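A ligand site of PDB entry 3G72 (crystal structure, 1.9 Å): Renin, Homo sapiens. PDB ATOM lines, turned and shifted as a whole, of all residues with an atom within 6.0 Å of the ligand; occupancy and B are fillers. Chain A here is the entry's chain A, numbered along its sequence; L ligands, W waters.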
ATOM      1  N   THR A  18       4.636 -23.256  -7.370  1.00  0.00           N
ATOM      2  CA  THR A  18       5.619 -22.353  -6.787  1.00  0.00           C
ATOM      3  C   THR A  18       6.748 -21.813  -7.676  1.00  0.00           C
ATOM      4  O   THR A  18       7.424 -20.864  -7.298  1.00  0.00           O
ATOM      5  CB  THR A  18       6.273 -22.997  -5.562  1.00  0.00           C
ATOM      6  OG1 THR A  18       6.796 -24.276  -5.947  1.00  0.00           O
ATOM      7  CG2 THR A  18       5.245 -23.310  -4.535  1.00  0.00           C
ATOM      8  N   GLN A  19       7.026 -22.485  -8.787  1.00  0.00           N
ATOM      9  CA  GLN A  19       8.116 -22.114  -9.677  1.00  0.00           C
ATOM     10  C   GLN A  19       7.528 -22.146 -11.067  1.00  0.00           C
ATOM     11  O   GLN A  19       6.974 -23.160 -11.477  1.00  0.00           O
ATOM     12  CB  GLN A  19       9.267 -23.140  -9.608  1.00  0.00           C
ATOM     13  CG  GLN A  19       9.893 -23.219  -8.208  1.00  0.00           C
ATOM     14  CD  GLN A  19      10.887 -24.326  -8.090  1.00  0.00           C
ATOM     15  OE1 GLN A  19      11.555 -24.691  -9.068  1.00  0.00           O
ATOM     16  NE2 GLN A  19      11.043 -24.835  -6.881  1.00  0.00           N
ATOM     17  N   VAL A  36      13.349 -18.298 -14.150  1.00  0.00           N
ATOM     18  CA  VAL A  36      12.179 -17.545 -13.707  1.00  0.00           C
ATOM     19  C   VAL A  36      12.316 -16.083 -14.221  1.00  0.00           C
ATOM     20  O   VAL A  36      13.394 -15.490 -14.140  1.00  0.00           O
ATOM     21  CB  VAL A  36      12.011 -17.669 -12.178  1.00  0.00           C
ATOM     22  CG1 VAL A  36      11.055 -16.544 -11.629  1.00  0.00           C
ATOM     23  CG2 VAL A  36      11.495 -19.058 -11.782  1.00  0.00           C
ATOM     24  N   ASP A  38      11.410 -12.548 -13.351  1.00  0.00           N
ATOM     25  CA  ASP A  38      11.173 -12.051 -12.002  1.00  0.00           C
ATOM     26  C   ASP A  38      11.053 -10.545 -12.045  1.00  0.00           C
ATOM     27  O   ASP A  38      12.032  -9.848 -12.216  1.00  0.00           O
ATOM     28  CB  ASP A  38      12.331 -12.515 -11.100  1.00  0.00           C
ATOM     29  CG  ASP A  38      12.226 -11.976  -9.669  1.00  0.00           C
ATOM     30  OD1 ASP A  38      11.141 -11.580  -9.271  1.00  0.00           O
ATOM     31  OD2 ASP A  38      13.205 -11.949  -8.854  1.00  0.00           O
ATOM     32  N   THR A  39       9.835 -10.021 -11.873  1.00  0.00           N
ATOM     33  CA  THR A  39       9.644  -8.572 -11.754  1.00  0.00           C
ATOM     34  C   THR A  39      10.213  -8.022 -10.425  1.00  0.00           C
ATOM     35  O   THR A  39      10.436  -6.838 -10.315  1.00  0.00           O
ATOM     36  CB  THR A  39       8.170  -8.183 -11.898  1.00  0.00           C
ATOM     37  OG1 THR A  39       7.430  -8.899 -10.915  1.00  0.00           O
ATOM     38  CG2 THR A  39       7.577  -8.680 -13.204  1.00  0.00           C
ATOM     39  N   GLY A  40      10.514  -8.885  -9.469  1.00  0.00           N
ATOM     40  CA  GLY A  40      11.113  -8.423  -8.223  1.00  0.00           C
ATOM     41  C   GLY A  40      12.617  -8.264  -8.255  1.00  0.00           C
ATOM     42  O   GLY A  40      13.265  -7.999  -7.221  1.00  0.00           O
ATOM     43  N   SER A  41      13.204  -8.439  -9.423  1.00  0.00           N
ATOM     44  CA  SER A  41      14.642  -8.362  -9.507  1.00  0.00           C
ATOM     45  C   SER A  41      15.069  -7.872 -10.859  1.00  0.00           C
ATOM     46  O   SER A  41      14.246  -7.793 -11.786  1.00  0.00           O
ATOM     47  CB  SER A  41      15.321  -9.664  -9.042  1.00  0.00           C
ATOM     48  OG  SER A  41      15.201 -10.731  -9.961  1.00  0.00           O
ATOM     49  N   TRP A  45      20.804 -13.790 -14.161  1.00  0.00           N
ATOM     50  CA  TRP A  45      21.785 -14.658 -13.523  1.00  0.00           C
ATOM     51  C   TRP A  45      21.619 -16.075 -14.040  1.00  0.00           C
ATOM     52  O   TRP A  45      20.500 -16.570 -14.047  1.00  0.00           O
ATOM     53  CB  TRP A  45      21.452 -14.791 -12.051  1.00  0.00           C
ATOM     54  CG  TRP A  45      21.591 -13.611 -11.216  1.00  0.00           C
ATOM     55  CD1 TRP A  45      20.611 -12.770 -10.859  1.00  0.00           C
ATOM     56  CD2 TRP A  45      22.762 -13.216 -10.496  1.00  0.00           C
ATOM     57  NE1 TRP A  45      21.104 -11.820  -9.991  1.00  0.00           N
ATOM     58  CE2 TRP A  45      22.428 -12.068  -9.764  1.00  0.00           C
ATOM     59  CE3 TRP A  45      24.081 -13.696 -10.436  1.00  0.00           C
ATOM     60  CZ2 TRP A  45      23.349 -11.386  -8.938  1.00  0.00           C
ATOM     61  CZ3 TRP A  45      25.027 -13.007  -9.637  1.00  0.00           C
ATOM     62  CH2 TRP A  45      24.626 -11.865  -8.880  1.00  0.00           C
ATOM     63  N   VAL A  46      22.701 -16.721 -14.441  1.00  0.00           N
ATOM     64  CA  VAL A  46      22.681 -18.167 -14.598  1.00  0.00           C
ATOM     65  C   VAL A  46      23.882 -18.744 -13.851  1.00  0.00           C
ATOM     66  O   VAL A  46      24.845 -18.013 -13.571  1.00  0.00           O
ATOM     67  CB  VAL A  46      22.737 -18.618 -16.086  1.00  0.00           C
ATOM     68  CG1 VAL A  46      21.460 -18.198 -16.816  1.00  0.00           C
ATOM     69  CG2 VAL A  46      23.944 -18.114 -16.743  1.00  0.00           C
ATOM     70  N   PRO A  47      23.869 -20.027 -13.569  1.00  0.00           N
ATOM     71  CA  PRO A  47      25.053 -20.653 -12.949  1.00  0.00           C
ATOM     72  C   PRO A  47      26.214 -20.654 -13.953  1.00  0.00           C
ATOM     73  O   PRO A  47      26.000 -20.915 -15.160  1.00  0.00           O
ATOM     74  CB  PRO A  47      24.611 -22.073 -12.680  1.00  0.00           C
ATOM     75  CG  PRO A  47      23.103 -22.099 -12.892  1.00  0.00           C
ATOM     76  CD  PRO A  47      22.809 -21.017 -13.864  1.00  0.00           C
ATOM     77  N   ALA A  57      23.628 -26.687  -5.541  1.00  0.00           N
ATOM     78  CA  ALA A  57      22.860 -25.866  -6.467  1.00  0.00           C
ATOM     79  C   ALA A  57      23.504 -25.818  -7.856  1.00  0.00           C
ATOM     80  O   ALA A  57      22.800 -25.648  -8.865  1.00  0.00           O
ATOM     81  CB  ALA A  57      22.713 -24.478  -5.923  1.00  0.00           C
ATOM     82  N   CYS A  58      24.821 -25.947  -7.932  1.00  0.00           N
ATOM     83  CA  CYS A  58      25.436 -25.943  -9.250  1.00  0.00           C
ATOM     84  C   CYS A  58      25.383 -27.311  -9.876  1.00  0.00           C
ATOM     85  O   CYS A  58      25.179 -27.432 -11.074  1.00  0.00           O
ATOM     86  CB  CYS A  58      26.870 -25.436  -9.208  1.00  0.00           C
ATOM     87  SG  CYS A  58      26.836 -23.660  -8.949  1.00  0.00           S
ATOM     88  N   HIS A  61      22.157 -28.126 -11.772  1.00  0.00           N
ATOM     89  CA  HIS A  61      21.677 -27.157 -12.728  1.00  0.00           C
ATOM     90  C   HIS A  61      22.565 -27.106 -13.974  1.00  0.00           C
ATOM     91  O   HIS A  61      23.683 -27.635 -13.981  1.00  0.00           O
ATOM     92  CB  HIS A  61      21.493 -25.788 -12.062  1.00  0.00           C
ATOM     93  CG  HIS A  61      20.334 -25.760 -11.101  1.00  0.00           C
ATOM     94  ND1 HIS A  61      20.483 -25.595  -9.740  1.00  0.00           N
ATOM     95  CD2 HIS A  61      19.004 -25.952 -11.309  1.00  0.00           C
ATOM     96  CE1 HIS A  61      19.305 -25.654  -9.149  1.00  0.00           C
ATOM     97  NE2 HIS A  61      18.385 -25.882 -10.076  1.00  0.00           N
ATOM     98  N   LEU A  81      24.624 -10.868  -4.561  1.00  0.00           N
ATOM     99  CA  LEU A  81      23.316 -10.740  -3.945  1.00  0.00           C
ATOM    100  C   LEU A  81      23.381 -11.383  -2.554  1.00  0.00           C
ATOM    101  O   LEU A  81      23.696 -12.585  -2.387  1.00  0.00           O
ATOM    102  CB  LEU A  81      22.265 -11.440  -4.803  1.00  0.00           C
ATOM    103  CG  LEU A  81      20.782 -11.160  -4.528  1.00  0.00           C
ATOM    104  CD1 LEU A  81      19.941 -12.070  -5.406  1.00  0.00           C
ATOM    105  CD2 LEU A  81      20.422 -11.426  -3.102  1.00  0.00           C
ATOM    106  N   TYR A  83      21.438 -12.906  -0.239  1.00  0.00           N
ATOM    107  CA  TYR A  83      20.162 -13.607  -0.118  1.00  0.00           C
ATOM    108  C   TYR A  83      19.946 -14.035   1.349  1.00  0.00           C
ATOM    109  O   TYR A  83      20.914 -14.143   2.094  1.00  0.00           O
ATOM    110  CB  TYR A  83      20.161 -14.801  -1.073  1.00  0.00           C
ATOM    111  CG  TYR A  83      18.863 -15.512  -1.100  1.00  0.00           C
ATOM    112  CD1 TYR A  83      18.698 -16.709  -0.392  1.00  0.00           C
ATOM    113  CD2 TYR A  83      17.782 -14.986  -1.797  1.00  0.00           C
ATOM    114  CE1 TYR A  83      17.493 -17.361  -0.381  1.00  0.00           C
ATOM    115  CE2 TYR A  83      16.553 -15.648  -1.800  1.00  0.00           C
ATOM    116  CZ  TYR A  83      16.429 -16.846  -1.091  1.00  0.00           C
ATOM    117  OH  TYR A  83      15.225 -17.507  -1.069  1.00  0.00           O
ATOM    118  N   VAL A  88      24.685 -15.096  -2.800  1.00  0.00           N
ATOM    119  CA  VAL A  88      24.770 -15.552  -4.202  1.00  0.00           C
ATOM    120  C   VAL A  88      25.783 -14.599  -4.858  1.00  0.00           C
ATOM    121  O   VAL A  88      25.683 -13.360  -4.693  1.00  0.00           O
ATOM    122  CB  VAL A  88      23.399 -15.511  -4.949  1.00  0.00           C
ATOM    123  CG1 VAL A  88      23.583 -15.787  -6.455  1.00  0.00           C
ATOM    124  CG2 VAL A  88      22.440 -16.520  -4.362  1.00  0.00           C
ATOM    125  N   VAL A 111      26.853 -17.091 -11.854  1.00  0.00           N
ATOM    126  CA  VAL A 111      26.974 -17.484 -10.451  1.00  0.00           C
ATOM    127  C   VAL A 111      28.020 -18.566 -10.232  1.00  0.00           C
ATOM    128  O   VAL A 111      27.965 -19.661 -10.835  1.00  0.00           O
ATOM    129  CB  VAL A 111      25.636 -18.000  -9.878  1.00  0.00           C
ATOM    130  CG1 VAL A 111      25.774 -18.283  -8.321  1.00  0.00           C
ATOM    131  CG2 VAL A 111      24.522 -17.050 -10.145  1.00  0.00           C
ATOM    132  N   MET A 114      26.531 -20.116  -4.366  1.00  0.00           N
ATOM    133  CA  MET A 114      25.251 -19.749  -3.771  1.00  0.00           C
ATOM    134  C   MET A 114      24.860 -20.786  -2.759  1.00  0.00           C
ATOM    135  O   MET A 114      25.371 -21.899  -2.794  1.00  0.00           O
ATOM    136  CB  MET A 114      24.183 -19.715  -4.878  1.00  0.00           C
ATOM    137  CG  MET A 114      24.003 -21.044  -5.582  1.00  0.00           C
ATOM    138  SD  MET A 114      22.965 -20.887  -7.063  1.00  0.00           S
ATOM    139  CE  MET A 114      22.146 -19.352  -6.735  1.00  0.00           C
ATOM    140  N   PRO A 118      17.687 -21.893  -0.953  1.00  0.00           N
ATOM    141  CA  PRO A 118      16.747 -22.843  -1.613  1.00  0.00           C
ATOM    142  C   PRO A 118      17.115 -23.319  -3.022  1.00  0.00           C
ATOM    143  O   PRO A 118      16.369 -24.062  -3.634  1.00  0.00           O
ATOM    144  CB  PRO A 118      15.479 -21.996  -1.708  1.00  0.00           C
ATOM    145  CG  PRO A 118      15.967 -20.598  -1.852  1.00  0.00           C
ATOM    146  CD  PRO A 118      17.295 -20.490  -1.146  1.00  0.00           C
ATOM    147  N   PHE A 119      18.271 -22.901  -3.509  1.00  0.00           N
ATOM    148  CA  PHE A 119      18.656 -23.076  -4.910  1.00  0.00           C
ATOM    149  C   PHE A 119      18.735 -24.495  -5.479  1.00  0.00           C
ATOM    150  O   PHE A 119      18.435 -24.712  -6.671  1.00  0.00           O
ATOM    151  CB  PHE A 119      19.891 -22.233  -5.166  1.00  0.00           C
ATOM    152  CG  PHE A 119      19.687 -20.802  -4.756  1.00  0.00           C
ATOM    153  CD1 PHE A 119      18.871 -19.969  -5.530  1.00  0.00           C
ATOM    154  CD2 PHE A 119      20.206 -20.310  -3.557  1.00  0.00           C
ATOM    155  CE1 PHE A 119      18.653 -18.660  -5.160  1.00  0.00           C
ATOM    156  CE2 PHE A 119      19.991 -18.991  -3.178  1.00  0.00           C
ATOM    157  CZ  PHE A 119      19.212 -18.151  -3.970  1.00  0.00           C
ATOM    158  N   MET A 120      19.155 -25.462  -4.664  1.00  0.00           N
ATOM    159  CA  MET A 120      19.189 -26.861  -5.112  1.00  0.00           C
ATOM    160  C   MET A 120      17.775 -27.419  -5.288  1.00  0.00           C
ATOM    161  O   MET A 120      17.615 -28.468  -5.861  1.00  0.00           O
ATOM    162  CB  MET A 120      19.944 -27.757  -4.127  1.00  0.00           C
ATOM    163  CG  MET A 120      19.089 -28.153  -2.936  1.00  0.00           C
ATOM    164  SD  MET A 120      19.979 -29.048  -1.601  1.00  0.00           S
ATOM    165  CE  MET A 120      19.953 -30.686  -2.328  1.00  0.00           C
ATOM    166  N   LEU A 121      16.758 -26.697  -4.792  1.00  0.00           N
ATOM    167  CA  LEU A 121      15.332 -27.100  -4.915  1.00  0.00           C
ATOM    168  C   LEU A 121      14.621 -26.452  -6.118  1.00  0.00           C
ATOM    169  O   LEU A 121      13.527 -26.857  -6.515  1.00  0.00           O
ATOM    170  CB  LEU A 121      14.565 -26.780  -3.616  1.00  0.00           C
ATOM    171  CG  LEU A 121      15.230 -27.434  -2.382  1.00  0.00           C
ATOM    172  CD1 LEU A 121      14.534 -27.063  -1.051  1.00  0.00           C
ATOM    173  CD2 LEU A 121      15.295 -28.924  -2.564  1.00  0.00           C
ATOM    174  N   ALA A 122      15.278 -25.452  -6.682  1.00  0.00           N
ATOM    175  CA  ALA A 122      14.818 -24.814  -7.907  1.00  0.00           C
ATOM    176  C   ALA A 122      14.844 -25.803  -9.076  1.00  0.00           C
ATOM    177  O   ALA A 122      15.885 -26.418  -9.338  1.00  0.00           O
ATOM    178  CB  ALA A 122      15.717 -23.630  -8.185  1.00  0.00           C
ATOM    179  N   GLU A 123      13.719 -25.997  -9.767  1.00  0.00           N
ATOM    180  CA  GLU A 123      13.691 -26.817 -10.988  1.00  0.00           C
ATOM    181  C   GLU A 123      14.260 -26.039 -12.163  1.00  0.00           C
ATOM    182  O   GLU A 123      14.627 -26.625 -13.165  1.00  0.00           O
ATOM    183  CB  GLU A 123      12.274 -27.324 -11.289  1.00  0.00           C
ATOM    184  CG  GLU A 123      11.721 -28.187 -10.163  1.00  0.00           C
ATOM    185  CD  GLU A 123      12.284 -29.601 -10.179  1.00  0.00           C
ATOM    186  OE1 GLU A 123      12.560 -30.151 -11.276  1.00  0.00           O
ATOM    187  OE2 GLU A 123      12.466 -30.168  -9.074  1.00  0.00           O
ATOM    188  N   PHE A 124      14.357 -24.726 -12.004  1.00  0.00           N
ATOM    189  CA  PHE A 124      14.992 -23.835 -12.986  1.00  0.00           C
ATOM    190  C   PHE A 124      16.468 -23.568 -12.640  1.00  0.00           C
ATOM    191  O   PHE A 124      16.905 -23.759 -11.481  1.00  0.00           O
ATOM    192  CB  PHE A 124      14.204 -22.514 -13.101  1.00  0.00           C
ATOM    193  CG  PHE A 124      14.035 -21.809 -11.770  1.00  0.00           C
ATOM    194  CD1 PHE A 124      13.078 -22.243 -10.862  1.00  0.00           C
ATOM    195  CD2 PHE A 124      14.897 -20.758 -11.407  1.00  0.00           C
ATOM    196  CE1 PHE A 124      12.949 -21.606  -9.617  1.00  0.00           C
ATOM    197  CE2 PHE A 124      14.757 -20.101 -10.171  1.00  0.00           C
ATOM    198  CZ  PHE A 124      13.796 -20.547  -9.283  1.00  0.00           C
ATOM    199  N   ASP A 125      17.220 -23.124 -13.648  1.00  0.00           N
ATOM    200  CA  ASP A 125      18.656 -22.856 -13.591  1.00  0.00           C
ATOM    201  C   ASP A 125      18.965 -21.416 -13.228  1.00  0.00           C
ATOM    202  O   ASP A 125      20.020 -21.101 -12.704  1.00  0.00           O
ATOM    203  CB  ASP A 125      19.276 -23.108 -14.975  1.00  0.00           C
ATOM    204  CG  ASP A 125      18.898 -24.451 -15.544  1.00  0.00           C
ATOM    205  OD1 ASP A 125      19.237 -25.470 -14.914  1.00  0.00           O
ATOM    206  OD2 ASP A 125      18.275 -24.571 -16.644  1.00  0.00           O
ATOM    207  N   GLY A 126      18.086 -20.500 -13.584  1.00  0.00           N
ATOM    208  CA  GLY A 126      18.453 -19.125 -13.415  1.00  0.00           C
ATOM    209  C   GLY A 126      17.303 -18.157 -13.317  1.00  0.00           C
ATOM    210  O   GLY A 126      16.121 -18.565 -13.255  1.00  0.00           O
ATOM    211  N   VAL A 127      17.620 -16.870 -13.274  1.00  0.00           N
ATOM    212  CA  VAL A 127      16.604 -15.827 -13.189  1.00  0.00           C
ATOM    213  C   VAL A 127      16.834 -14.593 -14.036  1.00  0.00           C
ATOM    214  O   VAL A 127      17.858 -13.917 -13.939  1.00  0.00           O
ATOM    215  CB  VAL A 127      16.254 -15.389 -11.731  1.00  0.00           C
ATOM    216  CG1 VAL A 127      17.305 -15.834 -10.756  1.00  0.00           C
ATOM    217  CG2 VAL A 127      15.926 -13.886 -11.637  1.00  0.00           C
ATOM    218  N   LEU A 224       4.541  -4.948  -3.712  1.00  0.00           N
ATOM    219  CA  LEU A 224       5.460  -5.316  -4.763  1.00  0.00           C
ATOM    220  C   LEU A 224       4.763  -6.397  -5.599  1.00  0.00           C
ATOM    221  O   LEU A 224       4.241  -7.342  -5.037  1.00  0.00           O
ATOM    222  CB  LEU A 224       6.778  -5.827  -4.158  1.00  0.00           C
ATOM    223  CG  LEU A 224       7.851  -6.354  -5.119  1.00  0.00           C
ATOM    224  CD1 LEU A 224       8.439  -5.213  -5.994  1.00  0.00           C
ATOM    225  CD2 LEU A 224       8.981  -7.043  -4.298  1.00  0.00           C
ATOM    226  N   ASP A 226       5.510  -9.312  -7.818  1.00  0.00           N
ATOM    227  CA  ASP A 226       6.767 -10.028  -7.853  1.00  0.00           C
ATOM    228  C   ASP A 226       6.586 -11.400  -8.452  1.00  0.00           C
ATOM    229  O   ASP A 226       6.222 -12.362  -7.768  1.00  0.00           O
ATOM    230  CB  ASP A 226       7.286 -10.112  -6.421  1.00  0.00           C
ATOM    231  CG  ASP A 226       8.683 -10.691  -6.310  1.00  0.00           C
ATOM    232  OD1 ASP A 226       9.301 -11.185  -7.299  1.00  0.00           O
ATOM    233  OD2 ASP A 226       9.273 -10.680  -5.196  1.00  0.00           O
ATOM    234  N   THR A 227       6.807 -11.514  -9.771  1.00  0.00           N
ATOM    235  CA  THR A 227       6.475 -12.739 -10.491  1.00  0.00           C
ATOM    236  C   THR A 227       7.386 -13.883 -10.076  1.00  0.00           C
ATOM    237  O   THR A 227       7.082 -15.045 -10.334  1.00  0.00           O
ATOM    238  CB  THR A 227       6.616 -12.491 -11.981  1.00  0.00           C
ATOM    239  OG1 THR A 227       7.930 -11.921 -12.235  1.00  0.00           O
ATOM    240  CG2 THR A 227       5.593 -11.397 -12.431  1.00  0.00           C
ATOM    241  N   GLY A 228       8.518 -13.506  -9.490  1.00  0.00           N
ATOM    242  CA  GLY A 228       9.520 -14.458  -9.025  1.00  0.00           C
ATOM    243  C   GLY A 228       9.207 -15.010  -7.652  1.00  0.00           C
ATOM    244  O   GLY A 228       9.882 -15.945  -7.241  1.00  0.00           O
ATOM    245  N   ALA A 229       8.242 -14.413  -6.924  1.00  0.00           N
ATOM    246  CA  ALA A 229       7.809 -14.915  -5.601  1.00  0.00           C
ATOM    247  C   ALA A 229       6.735 -15.987  -5.794  1.00  0.00           C
ATOM    248  O   ALA A 229       5.814 -15.780  -6.535  1.00  0.00           O
ATOM    249  CB  ALA A 229       7.269 -13.740  -4.734  1.00  0.00           C
ATOM    250  N   SER A 230       6.871 -17.136  -5.122  1.00  0.00           N
ATOM    251  CA  SER A 230       5.858 -18.200  -5.176  1.00  0.00           C
ATOM    252  C   SER A 230       4.479 -17.820  -4.571  1.00  0.00           C
ATOM    253  O   SER A 230       3.395 -18.231  -5.062  1.00  0.00           O
ATOM    254  CB  SER A 230       6.401 -19.406  -4.402  1.00  0.00           C
ATOM    255  OG  SER A 230       7.604 -19.906  -4.941  1.00  0.00           O
ATOM    256  N   MET A 303       7.209 -12.398   5.116  1.00  0.00           N
ATOM    257  CA  MET A 303       8.547 -12.013   4.674  1.00  0.00           C
ATOM    258  C   MET A 303       8.800 -10.539   4.912  1.00  0.00           C
ATOM    259  O   MET A 303       8.089  -9.671   4.391  1.00  0.00           O
ATOM    260  CB  MET A 303       8.768 -12.357   3.216  1.00  0.00           C
ATOM    261  CG  MET A 303      10.151 -11.999   2.705  1.00  0.00           C
ATOM    262  SD  MET A 303      10.438 -12.681   1.050  1.00  0.00           S
ATOM    263  CE  MET A 303      10.369 -14.447   1.417  1.00  0.00           C
HETATM  264  C1  LIG L   1      11.367 -13.269  -5.643  1.00  0.00           C
HETATM  265 CL1  LIG L   1      13.357 -22.769  -5.284  1.00  0.00          CL
HETATM  266  C2  LIG L   1      12.813 -21.096  -5.433  1.00  0.00           C
HETATM  267  C3  LIG L   1      13.760 -20.138  -5.625  1.00  0.00           C
HETATM  268 CL2  LIG L   1      15.492 -20.559  -5.656  1.00  0.00          CL
HETATM  269  C4  LIG L   1      11.456 -20.778  -5.392  1.00  0.00           C
HETATM  270  C5  LIG L   1      11.086 -19.460  -5.513  1.00  0.00           C
HETATM  271  C6  LIG L   1      12.055 -18.483  -5.701  1.00  0.00           C
HETATM  272  C7  LIG L   1      13.401 -18.811  -5.739  1.00  0.00           C
HETATM  273  C8  LIG L   1      14.526 -17.807  -5.920  1.00  0.00           C
HETATM  274  N1  LIG L   1      14.225 -16.415  -6.215  1.00  0.00           N
HETATM  275  C9  LIG L   1      14.393 -16.014  -7.659  1.00  0.00           C
HETATM  276  C10 LIG L   1      13.519 -16.884  -8.564  1.00  0.00           C
HETATM  277  C11 LIG L   1      13.131 -15.441  -8.352  1.00  0.00           C
HETATM  278  C12 LIG L   1      13.969 -15.588  -5.180  1.00  0.00           C
HETATM  279  O1  LIG L   1      13.913 -16.034  -4.023  1.00  0.00           O
HETATM  280  C13 LIG L   1      13.754 -14.153  -5.270  1.00  0.00           C
HETATM  281  C14 LIG L   1      12.509 -13.566  -4.656  1.00  0.00           C
HETATM  282  N2  LIG L   1      12.962 -12.339  -3.993  1.00  0.00           N
HETATM  283  C15 LIG L   1      13.428 -11.329  -4.937  1.00  0.00           C
HETATM  284  C16 LIG L   1      14.573 -11.831  -5.802  1.00  0.00           C
HETATM  285  N3  LIG L   1      11.636 -12.095  -6.484  1.00  0.00           N
HETATM  286  C17 LIG L   1      12.255 -10.955  -5.840  1.00  0.00           C
HETATM  287  C18 LIG L   1      14.720 -13.359  -5.773  1.00  0.00           C
HETATM  288  C19 LIG L   1      16.037 -13.813  -6.319  1.00  0.00           C
HETATM  289  C20 LIG L   1      16.846 -14.625  -5.535  1.00  0.00           C
HETATM  290  C21 LIG L   1      18.105 -15.020  -5.980  1.00  0.00           C
HETATM  291  C22 LIG L   1      16.505 -13.338  -7.566  1.00  0.00           C
HETATM  292  C23 LIG L   1      17.774 -13.723  -8.014  1.00  0.00           C
HETATM  293  C24 LIG L   1      18.587 -14.554  -7.209  1.00  0.00           C
HETATM  294  C25 LIG L   1      19.938 -14.981  -7.641  1.00  0.00           C
HETATM  295  C26 LIG L   1      20.055 -15.736  -8.722  1.00  0.00           C
HETATM  296  C27 LIG L   1      19.695 -17.173  -8.500  1.00  0.00           C
HETATM  297  O2  LIG L   1      19.771 -17.867  -9.741  1.00  0.00           O
HETATM  298  C28 LIG L   1      19.442 -19.186  -9.543  1.00  0.00           C
HETATM  299  C29 LIG L   1      18.192 -19.592  -9.067  1.00  0.00           C
HETATM  300  F1  LIG L   1      17.264 -18.684  -8.726  1.00  0.00           F
HETATM  301  C30 LIG L   1      20.379 -20.125  -9.884  1.00  0.00           C
HETATM  302 CL3  LIG L   1      21.936 -19.513 -10.551  1.00  0.00          CL
HETATM  303  C31 LIG L   1      20.074 -21.477  -9.710  1.00  0.00           C
HETATM  304  F2  LIG L   1      20.954 -22.422 -10.029  1.00  0.00           F
HETATM  305  C32 LIG L   1      18.848 -21.882  -9.219  1.00  0.00           C
HETATM  306  C33 LIG L   1      17.905 -20.935  -8.908  1.00  0.00           C
HETATM  307  O   HOH W   1      16.592 -10.173  -3.614  1.00  0.00           O
HETATM  308  O   HOH W   2      11.518 -10.484  -2.324  1.00  0.00           O
HETATM  309  O   HOH W   3      15.480 -12.417  -2.688  1.00  0.00           O
HETATM  310  O   HOH W   4      10.505 -14.668  -2.244  1.00  0.00           O
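N3 of the ligand is in salt-bridge range of OD1 of Asp 226 (2.6 Å).
The side-chain carboxylate (OD2) of Asp 38 is in salt-bridge range of a nitrogen (N3) of the ligand (2.8 Å).
N of Gly 40 is in hydrogen-bond range of OD1 of Asp 226, 3.4 Å away.
OD1 of Asp 226 sits close to N of Gly 228, 3.3 Å away.
The side-chain carboxylate (OD1) of Asp 38 lies within hydrogen-bond range of the backbone NH (N) of Gly 40, at 2.8 Å.
OD1 of Asp 38 sits at hydrogen-bond distance from N of Gly 228 (3.3 Å).
A ring nitrogen (NE2) of His 61 lies within hydrogen-bond range of the backbone carbonyl oxygen of Ala 122, at 2.7 Å.
The backbone carbonyl oxygen of Val 127 sits at hydrogen-bond distance from the backbone NH of Trp 45 (3.0 Å).
The side-chain amide nitrogen of Gln 19 is in hydrogen-bond range of the backbone carbonyl oxygen of Leu 121 (3.2 Å).
OG of Ser 230 lies within hydrogen-bond range of O of Thr 18, 2.6 Å away.
ND1 of His 61 sits close to F2 of the ligand (3.2 Å).
A fluorine (F2) of the ligand lies close to the backbone carbonyl oxygen (O) of Asp 125 (3.1 Å).
Merely in contact with the ligand: Phe 124 (3.2 Å), Val 127 (3.4 Å), Leu 81 (3.4 Å), Gly 40 (3.4 Å), Gly 228 (3.4 Å), Phe 119 (3.4 Å), Tyr 83 (3.5 Å), Gln 19 (3.5 Å), Ala 122 (3.5 Å), Ser 230 (3.6 Å), Ala 229 (3.6 Å), Val 111 (3.6 Å), Pro 47 (3.6 Å), Trp 45 (3.6 Å), Pro 118 (3.7 Å), Met 114 (3.7 Å), Ser 41 (3.8 Å), Ala 57 (3.9 Å), Val 46 (3.9 Å), Val 88 (3.9 Å), Val 36 (3.9 Å), Leu 121 (3.98 Å) and Gly 126 (3.997 Å).
Hydrophobic or aromatic side chains within 4 Å of the ligand: Val 36, Trp 45, Pro 47, His 61, Leu 81, Tyr 83, Val 88, Val 111, Met 114, Pro 118, Phe 119, Ala 122, Phe 124 and Val 127.
Of the 35 residues printed, 27 come within 4 Å of the ligand.
Along chain A the residues within 4 Å of the ligand span positions 19 to 230.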
